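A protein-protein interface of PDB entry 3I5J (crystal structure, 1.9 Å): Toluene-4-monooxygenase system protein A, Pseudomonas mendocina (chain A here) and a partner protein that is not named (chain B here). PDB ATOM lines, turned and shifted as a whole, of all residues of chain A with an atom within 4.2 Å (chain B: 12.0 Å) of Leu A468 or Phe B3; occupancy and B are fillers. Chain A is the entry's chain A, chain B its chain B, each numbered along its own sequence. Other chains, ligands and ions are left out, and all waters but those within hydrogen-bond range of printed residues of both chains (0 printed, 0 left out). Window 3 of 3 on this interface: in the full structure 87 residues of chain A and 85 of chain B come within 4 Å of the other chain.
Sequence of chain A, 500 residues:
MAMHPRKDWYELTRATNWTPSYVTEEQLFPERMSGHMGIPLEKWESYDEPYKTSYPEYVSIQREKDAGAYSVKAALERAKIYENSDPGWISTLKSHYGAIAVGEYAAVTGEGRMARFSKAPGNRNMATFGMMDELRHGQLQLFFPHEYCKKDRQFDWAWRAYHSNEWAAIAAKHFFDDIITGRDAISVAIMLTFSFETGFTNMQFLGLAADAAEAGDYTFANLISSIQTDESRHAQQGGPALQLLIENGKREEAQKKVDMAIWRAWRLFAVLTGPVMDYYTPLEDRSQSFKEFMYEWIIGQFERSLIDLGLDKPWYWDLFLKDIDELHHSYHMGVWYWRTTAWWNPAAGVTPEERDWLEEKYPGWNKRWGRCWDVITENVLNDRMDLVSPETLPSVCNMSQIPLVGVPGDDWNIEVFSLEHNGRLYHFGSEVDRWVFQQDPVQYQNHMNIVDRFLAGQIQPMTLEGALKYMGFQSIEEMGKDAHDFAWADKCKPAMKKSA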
ATOM      1  N   THR A 340     -14.958 -13.448  18.091  1.00  0.00           N
ATOM      2  CA  THR A 340     -13.960 -13.328  17.020  1.00  0.00           C
ATOM      3  C   THR A 340     -14.533 -13.608  15.581  1.00  0.00           C
ATOM      4  O   THR A 340     -13.964 -13.172  14.578  1.00  0.00           O
ATOM      5  CB  THR A 340     -12.758 -14.227  17.371  1.00  0.00           C
ATOM      6  OG1 THR A 340     -11.729 -13.925  16.432  1.00  0.00           O
ATOM      7  CG2 THR A 340     -13.150 -15.703  17.330  1.00  0.00           C
ATOM      8  N   THR A 341     -15.683 -14.265  15.471  1.00  0.00           N
ATOM      9  CA  THR A 341     -16.306 -14.496  14.181  1.00  0.00           C
ATOM     10  C   THR A 341     -17.339 -13.448  13.797  1.00  0.00           C
ATOM     11  O   THR A 341     -17.943 -13.566  12.737  1.00  0.00           O
ATOM     12  CB  THR A 341     -17.065 -15.872  14.121  1.00  0.00           C
ATOM     13  OG1 THR A 341     -18.157 -15.831  15.043  1.00  0.00           O
ATOM     14  CG2 THR A 341     -16.146 -17.052  14.446  1.00  0.00           C
ATOM     15  N   LEU A 464     -10.006 -23.057  13.051  1.00  0.00           N
ATOM     16  CA  LEU A 464     -10.780 -21.842  13.335  1.00  0.00           C
ATOM     17  C   LEU A 464     -10.257 -20.696  12.461  1.00  0.00           C
ATOM     18  O   LEU A 464     -11.044 -19.891  11.887  1.00  0.00           O
ATOM     19  CB  LEU A 464     -10.760 -21.451  14.826  1.00  0.00           C
ATOM     20  CG  LEU A 464     -11.152 -19.968  15.113  1.00  0.00           C
ATOM     21  CD1 LEU A 464     -12.691 -19.760  15.233  1.00  0.00           C
ATOM     22  CD2 LEU A 464     -10.354 -19.374  16.350  1.00  0.00           C
ATOM     23  N   GLU A 465      -8.944 -20.603  12.353  1.00  0.00           N
ATOM     24  CA  GLU A 465      -8.385 -19.568  11.503  1.00  0.00           C
ATOM     25  C   GLU A 465      -8.819 -19.726  10.040  1.00  0.00           C
ATOM     26  O   GLU A 465      -9.115 -18.704   9.371  1.00  0.00           O
ATOM     27  CB  GLU A 465      -6.848 -19.533  11.536  1.00  0.00           C
ATOM     28  CG  GLU A 465      -6.353 -18.182  10.912  1.00  0.00           C
ATOM     29  CD  GLU A 465      -4.908 -17.854  11.236  1.00  0.00           C
ATOM     30  OE1 GLU A 465      -4.004 -18.348  10.529  1.00  0.00           O
ATOM     31  OE2 GLU A 465      -4.655 -17.080  12.182  1.00  0.00           O
ATOM     32  N   GLY A 466      -8.826 -20.972   9.538  1.00  0.00           N
ATOM     33  CA  GLY A 466      -9.271 -21.275   8.166  1.00  0.00           C
ATOM     34  C   GLY A 466     -10.742 -20.782   8.020  1.00  0.00           C
ATOM     35  O   GLY A 466     -11.139 -20.152   7.031  1.00  0.00           O
ATOM     36  N   ALA A 467     -11.558 -21.060   9.024  1.00  0.00           N
ATOM     37  CA  ALA A 467     -12.934 -20.557   9.005  1.00  0.00           C
ATOM     38  C   ALA A 467     -13.035 -19.005   9.061  1.00  0.00           C
ATOM     39  O   ALA A 467     -13.905 -18.402   8.377  1.00  0.00           O
ATOM     40  CB  ALA A 467     -13.747 -21.223  10.139  1.00  0.00           C
ATOM     41  N   LEU A 468     -12.236 -18.326   9.873  1.00  0.00           N
ATOM     42  CA  LEU A 468     -12.274 -16.854   9.898  1.00  0.00           C
ATOM     43  C   LEU A 468     -11.914 -16.301   8.525  1.00  0.00           C
ATOM     44  O   LEU A 468     -12.512 -15.363   8.037  1.00  0.00           O
ATOM     45  CB  LEU A 468     -11.328 -16.279  10.954  1.00  0.00           C
ATOM     46  CG  LEU A 468     -11.781 -16.564  12.386  1.00  0.00           C
ATOM     47  CD1 LEU A 468     -10.623 -16.410  13.432  1.00  0.00           C
ATOM     48  CD2 LEU A 468     -12.994 -15.671  12.656  1.00  0.00           C
ATOM     49  N   LYS A 469     -10.969 -16.923   7.855  1.00  0.00           N
ATOM     50  CA  LYS A 469     -10.603 -16.471   6.516  1.00  0.00           C
ATOM     51  C   LYS A 469     -11.714 -16.682   5.521  1.00  0.00           C
ATOM     52  O   LYS A 469     -12.074 -15.781   4.771  1.00  0.00           O
ATOM     53  CB  LYS A 469      -9.356 -17.221   6.034  1.00  0.00           C
ATOM     54  CG  LYS A 469      -8.108 -16.721   6.712  1.00  0.00           C
ATOM     55  CD  LYS A 469      -7.840 -15.268   6.365  1.00  0.00           C
ATOM     56  CE  LYS A 469      -6.323 -15.076   6.121  1.00  0.00           C
ATOM     57  NZ  LYS A 469      -5.520 -15.992   7.012  1.00  0.00           N
ATOM     58  N   TYR A 470     -12.303 -17.885   5.557  1.00  0.00           N
ATOM     59  CA  TYR A 470     -13.467 -18.205   4.744  1.00  0.00           C
ATOM     60  C   TYR A 470     -14.608 -17.213   4.934  1.00  0.00           C
ATOM     61  O   TYR A 470     -15.321 -16.862   3.991  1.00  0.00           O
ATOM     62  CB  TYR A 470     -13.920 -19.636   5.094  1.00  0.00           C
ATOM     63  CG  TYR A 470     -15.135 -20.062   4.346  1.00  0.00           C
ATOM     64  CD1 TYR A 470     -15.047 -20.506   3.017  1.00  0.00           C
ATOM     65  CD2 TYR A 470     -16.411 -20.003   4.951  1.00  0.00           C
ATOM     66  CE1 TYR A 470     -16.206 -20.921   2.329  1.00  0.00           C
ATOM     67  CE2 TYR A 470     -17.570 -20.394   4.253  1.00  0.00           C
ATOM     68  CZ  TYR A 470     -17.450 -20.840   2.943  1.00  0.00           C
ATOM     69  OH  TYR A 470     -18.595 -21.226   2.257  1.00  0.00           O
ATOM     70  N   MET A 471     -14.812 -16.776   6.175  1.00  0.00           N
ATOM     71  CA  MET A 471     -15.887 -15.830   6.492  1.00  0.00           C
ATOM     72  C   MET A 471     -15.626 -14.430   5.973  1.00  0.00           C
ATOM     73  O   MET A 471     -16.427 -13.542   6.140  1.00  0.00           O
ATOM     74  CB  MET A 471     -16.107 -15.793   8.022  1.00  0.00           C
ATOM     75  CG  MET A 471     -16.672 -17.136   8.599  1.00  0.00           C
ATOM     76  SD  MET A 471     -17.273 -16.855  10.292  1.00  0.00           S
ATOM     77  CE  MET A 471     -17.609 -18.529  10.703  1.00  0.00           C
ATOM     78  N   GLY A 472     -14.491 -14.205   5.350  1.00  0.00           N
ATOM     79  CA  GLY A 472     -14.263 -12.903   4.742  1.00  0.00           C
ATOM     80  C   GLY A 472     -13.432 -11.867   5.504  1.00  0.00           C
ATOM     81  O   GLY A 472     -13.258 -10.706   5.008  1.00  0.00           O
ATOM     82  N   PHE A 473     -12.959 -12.212   6.705  1.00  0.00           N
ATOM     83  CA  PHE A 473     -12.217 -11.209   7.480  1.00  0.00           C
ATOM     84  C   PHE A 473     -10.926 -10.895   6.764  1.00  0.00           C
ATOM     85  O   PHE A 473     -10.223 -11.825   6.377  1.00  0.00           O
ATOM     86  CB  PHE A 473     -11.974 -11.711   8.899  1.00  0.00           C
ATOM     87  CG  PHE A 473     -13.217 -11.734   9.697  1.00  0.00           C
ATOM     88  CD1 PHE A 473     -13.728 -10.538  10.188  1.00  0.00           C
ATOM     89  CD2 PHE A 473     -13.950 -12.907   9.825  1.00  0.00           C
ATOM     90  CE1 PHE A 473     -14.918 -10.514  10.880  1.00  0.00           C
ATOM     91  CE2 PHE A 473     -15.164 -12.899  10.525  1.00  0.00           C
ATOM     92  CZ  PHE A 473     -15.656 -11.702  11.051  1.00  0.00           C
ATOM     93  N   ILE A 476      -6.706  -8.307  11.152  1.00  0.00           N
ATOM     94  CA  ILE A 476      -6.917  -8.706  12.552  1.00  0.00           C
ATOM     95  C   ILE A 476      -7.898  -7.759  13.242  1.00  0.00           C
ATOM     96  O   ILE A 476      -8.677  -8.183  14.122  1.00  0.00           O
ATOM     97  CB  ILE A 476      -5.583  -8.792  13.369  1.00  0.00           C
ATOM     98  CG1 ILE A 476      -5.885  -9.228  14.800  1.00  0.00           C
ATOM     99  CG2 ILE A 476      -4.929  -7.497  13.420  1.00  0.00           C
ATOM    100  CD1 ILE A 476      -4.757 -10.033  15.447  1.00  0.00           C
ATOM    101  N   MET A 479     -11.979  -8.600  13.276  1.00  0.00           N
ATOM    102  CA  MET A 479     -12.678  -9.631  14.062  1.00  0.00           C
ATOM    103  C   MET A 479     -13.134  -9.094  15.435  1.00  0.00           C
ATOM    104  O   MET A 479     -12.406  -8.262  16.057  1.00  0.00           O
ATOM    105  CB  MET A 479     -11.782 -10.905  14.169  1.00  0.00           C
ATOM    106  CG  MET A 479     -11.155 -11.149  12.819  1.00  0.00           C
ATOM    107  SD  MET A 479     -10.215 -12.575  12.664  1.00  0.00           S
ATOM    108  CE  MET A 479      -8.594 -11.970  12.936  1.00  0.00           C
ATOM    109  N   SER B   2      -2.369 -16.479   7.592  1.00  0.00           N
ATOM    110  CA  SER B   2      -2.547 -15.701   8.851  1.00  0.00           C
ATOM    111  C   SER B   2      -3.133 -14.299   8.575  1.00  0.00           C
ATOM    112  O   SER B   2      -3.365 -13.924   7.411  1.00  0.00           O
ATOM    113  CB  SER B   2      -1.224 -15.592   9.566  1.00  0.00           C
ATOM    114  OG  SER B   2      -0.521 -14.484   9.035  1.00  0.00           O
ATOM    115  N   PHE B   3      -3.382 -13.534   9.640  1.00  0.00           N
ATOM    116  CA  PHE B   3      -4.064 -12.238   9.532  1.00  0.00           C
ATOM    117  C   PHE B   3      -3.109 -11.083   9.787  1.00  0.00           C
ATOM    118  O   PHE B   3      -2.400 -11.071  10.797  1.00  0.00           O
ATOM    119  CB  PHE B   3      -5.219 -12.138  10.518  1.00  0.00           C
ATOM    120  CG  PHE B   3      -6.418 -12.953  10.146  1.00  0.00           C
ATOM    121  CD1 PHE B   3      -7.355 -12.464   9.242  1.00  0.00           C
ATOM    122  CD2 PHE B   3      -6.635 -14.173  10.733  1.00  0.00           C
ATOM    123  CE1 PHE B   3      -8.479 -13.211   8.910  1.00  0.00           C
ATOM    124  CE2 PHE B   3      -7.759 -14.929  10.408  1.00  0.00           C
ATOM    125  CZ  PHE B   3      -8.683 -14.432   9.488  1.00  0.00           C
ATOM    126  N   GLU B   4      -3.069 -10.132   8.871  1.00  0.00           N
ATOM    127  CA  GLU B   4      -2.196  -8.983   9.075  1.00  0.00           C
ATOM    128  C   GLU B   4      -2.962  -7.817   9.618  1.00  0.00           C
ATOM    129  O   GLU B   4      -4.220  -7.787   9.634  1.00  0.00           O
ATOM    130  CB  GLU B   4      -1.527  -8.600   7.760  1.00  0.00           C
ATOM    131  CG  GLU B   4      -2.388  -8.827   6.494  1.00  0.00           C
ATOM    132  CD  GLU B   4      -1.572  -8.637   5.193  1.00  0.00           C
ATOM    133  OE1 GLU B   4      -1.054  -7.504   4.962  1.00  0.00           O
ATOM    134  OE2 GLU B   4      -1.453  -9.611   4.410  1.00  0.00           O
ATOM    135  N   SER B   5      -2.211  -6.824  10.062  1.00  0.00           N
ATOM    136  CA  SER B   5      -2.823  -5.601  10.488  1.00  0.00           C
ATOM    137  C   SER B   5      -2.972  -4.731   9.258  1.00  0.00           C
ATOM    138  O   SER B   5      -2.065  -4.661   8.421  1.00  0.00           O
ATOM    139  CB  SER B   5      -1.974  -4.930  11.574  1.00  0.00           C
ATOM    140  OG  SER B   5      -2.652  -3.810  12.134  1.00  0.00           O
ATOM    141  N   LYS B   6      -4.087  -4.036   9.159  1.00  0.00           N
ATOM    142  CA  LYS B   6      -4.285  -3.126   8.091  1.00  0.00           C
ATOM    143  C   LYS B   6      -4.990  -1.865   8.574  1.00  0.00           C
ATOM    144  O   LYS B   6      -5.832  -1.937   9.441  1.00  0.00           O
ATOM    145  CB  LYS B   6      -5.153  -3.779   7.014  1.00  0.00           C
ATOM    146  CG  LYS B   6      -4.546  -4.982   6.422  1.00  0.00           C
ATOM    147  CD  LYS B   6      -5.395  -5.487   5.337  1.00  0.00           C
ATOM    148  CE  LYS B   6      -4.555  -6.348   4.415  1.00  0.00           C
ATOM    149  NZ  LYS B   6      -5.398  -7.384   3.891  1.00  0.00           N
ATOM    150  N   LYS B   7      -4.683  -0.712   8.006  1.00  0.00           N
ATOM    151  CA  LYS B   7      -5.301   0.531   8.477  1.00  0.00           C
ATOM    152  C   LYS B   7      -6.743   0.704   7.985  1.00  0.00           C
ATOM    153  O   LYS B   7      -7.125   0.072   6.997  1.00  0.00           O
ATOM    154  CB  LYS B   7      -4.465   1.739   8.028  1.00  0.00           C
ATOM    155  CG  LYS B   7      -4.040   1.660   6.528  1.00  0.00           C
ATOM    156  CD  LYS B   7      -3.386   2.975   5.997  1.00  0.00           C
ATOM    157  CE  LYS B   7      -3.988   3.460   4.629  1.00  0.00           C
ATOM    158  NZ  LYS B   7      -3.116   4.493   3.943  1.00  0.00           N
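The side-chain amino group of Lys A469 lies within hydrogen-bond range of the backbone carbonyl oxygen of Ser B2 (3.0 Å). The backbone NH of Ile A476 is in hydrogen-bond range of the backbone carbonyl oxygen of Glu B4, 3.0 Å away.
N of Phe A473 sits close to O of Leu A468, 3.5 Å away.
Among the printed residues, pairs that only touch across the chains: Glu A465 with Ser B2, Glu A465 with Phe B3, Leu A468 with Phe B3, Lys A469 with Phe B3, Phe A473 with Phe B3 and Met A479 with Phe B3.
No residue of chain B comes within 4 Å of Thr A341. No residue of chain B comes within 4 Å of Leu A464. Of chain B, only Ser B2 and Phe B3 come within 4 Å of Glu A465. No residue of chain B comes within 4 Å of Gly A466. No residue of chain B comes within 4 Å of Ala A467. Leu A468 touches just one residue of chain B: Phe B3. Of chain B, only Ser B2 (3.0 Å) and Phe B3 (3.3 Å) come within 4 Å of Lys A469. No residue of chain B comes within 4 Å of Met A471. No residue of chain B comes within 4 Å of Gly A472. Phe A473 touches one residue of chain B. Ile A476 touches just one residue of chain B: Glu B4 (3.0 Å). Of the printed residues of chain B, Met A479 touches Phe B3. Of the printed residues of chain A, Ser B2 touches Glu A465 and Lys A469. Of chain A, only Glu A465 (3.6 Å), Leu A468 (3.5 Å), Lys A469 (3.3 Å), Phe A473 (3.4 Å) and Met A479 (3.7 Å) come within 4 Å of Phe B3. Printed residues of chain A within 4 Å of Glu B4: Ile A476. Lys B7 touches none of the printed residues of chain A. The nearest printed residue of chain A that does not touch Phe B3 is Ile A476 (4.2 Å).
Hydrophobic or aromatic side chains of chain A that line the printed part of chain B: Leu A468, Phe A473, Ile A476 and Met A479. Of the 6 printed residues of chain B, 3 touch a printed residue of chain A. Hydrophobic or aromatic side chains of chain B that line the printed part of chain A: Phe B3. Among the printed residues, 8 pairs touch across the chains.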
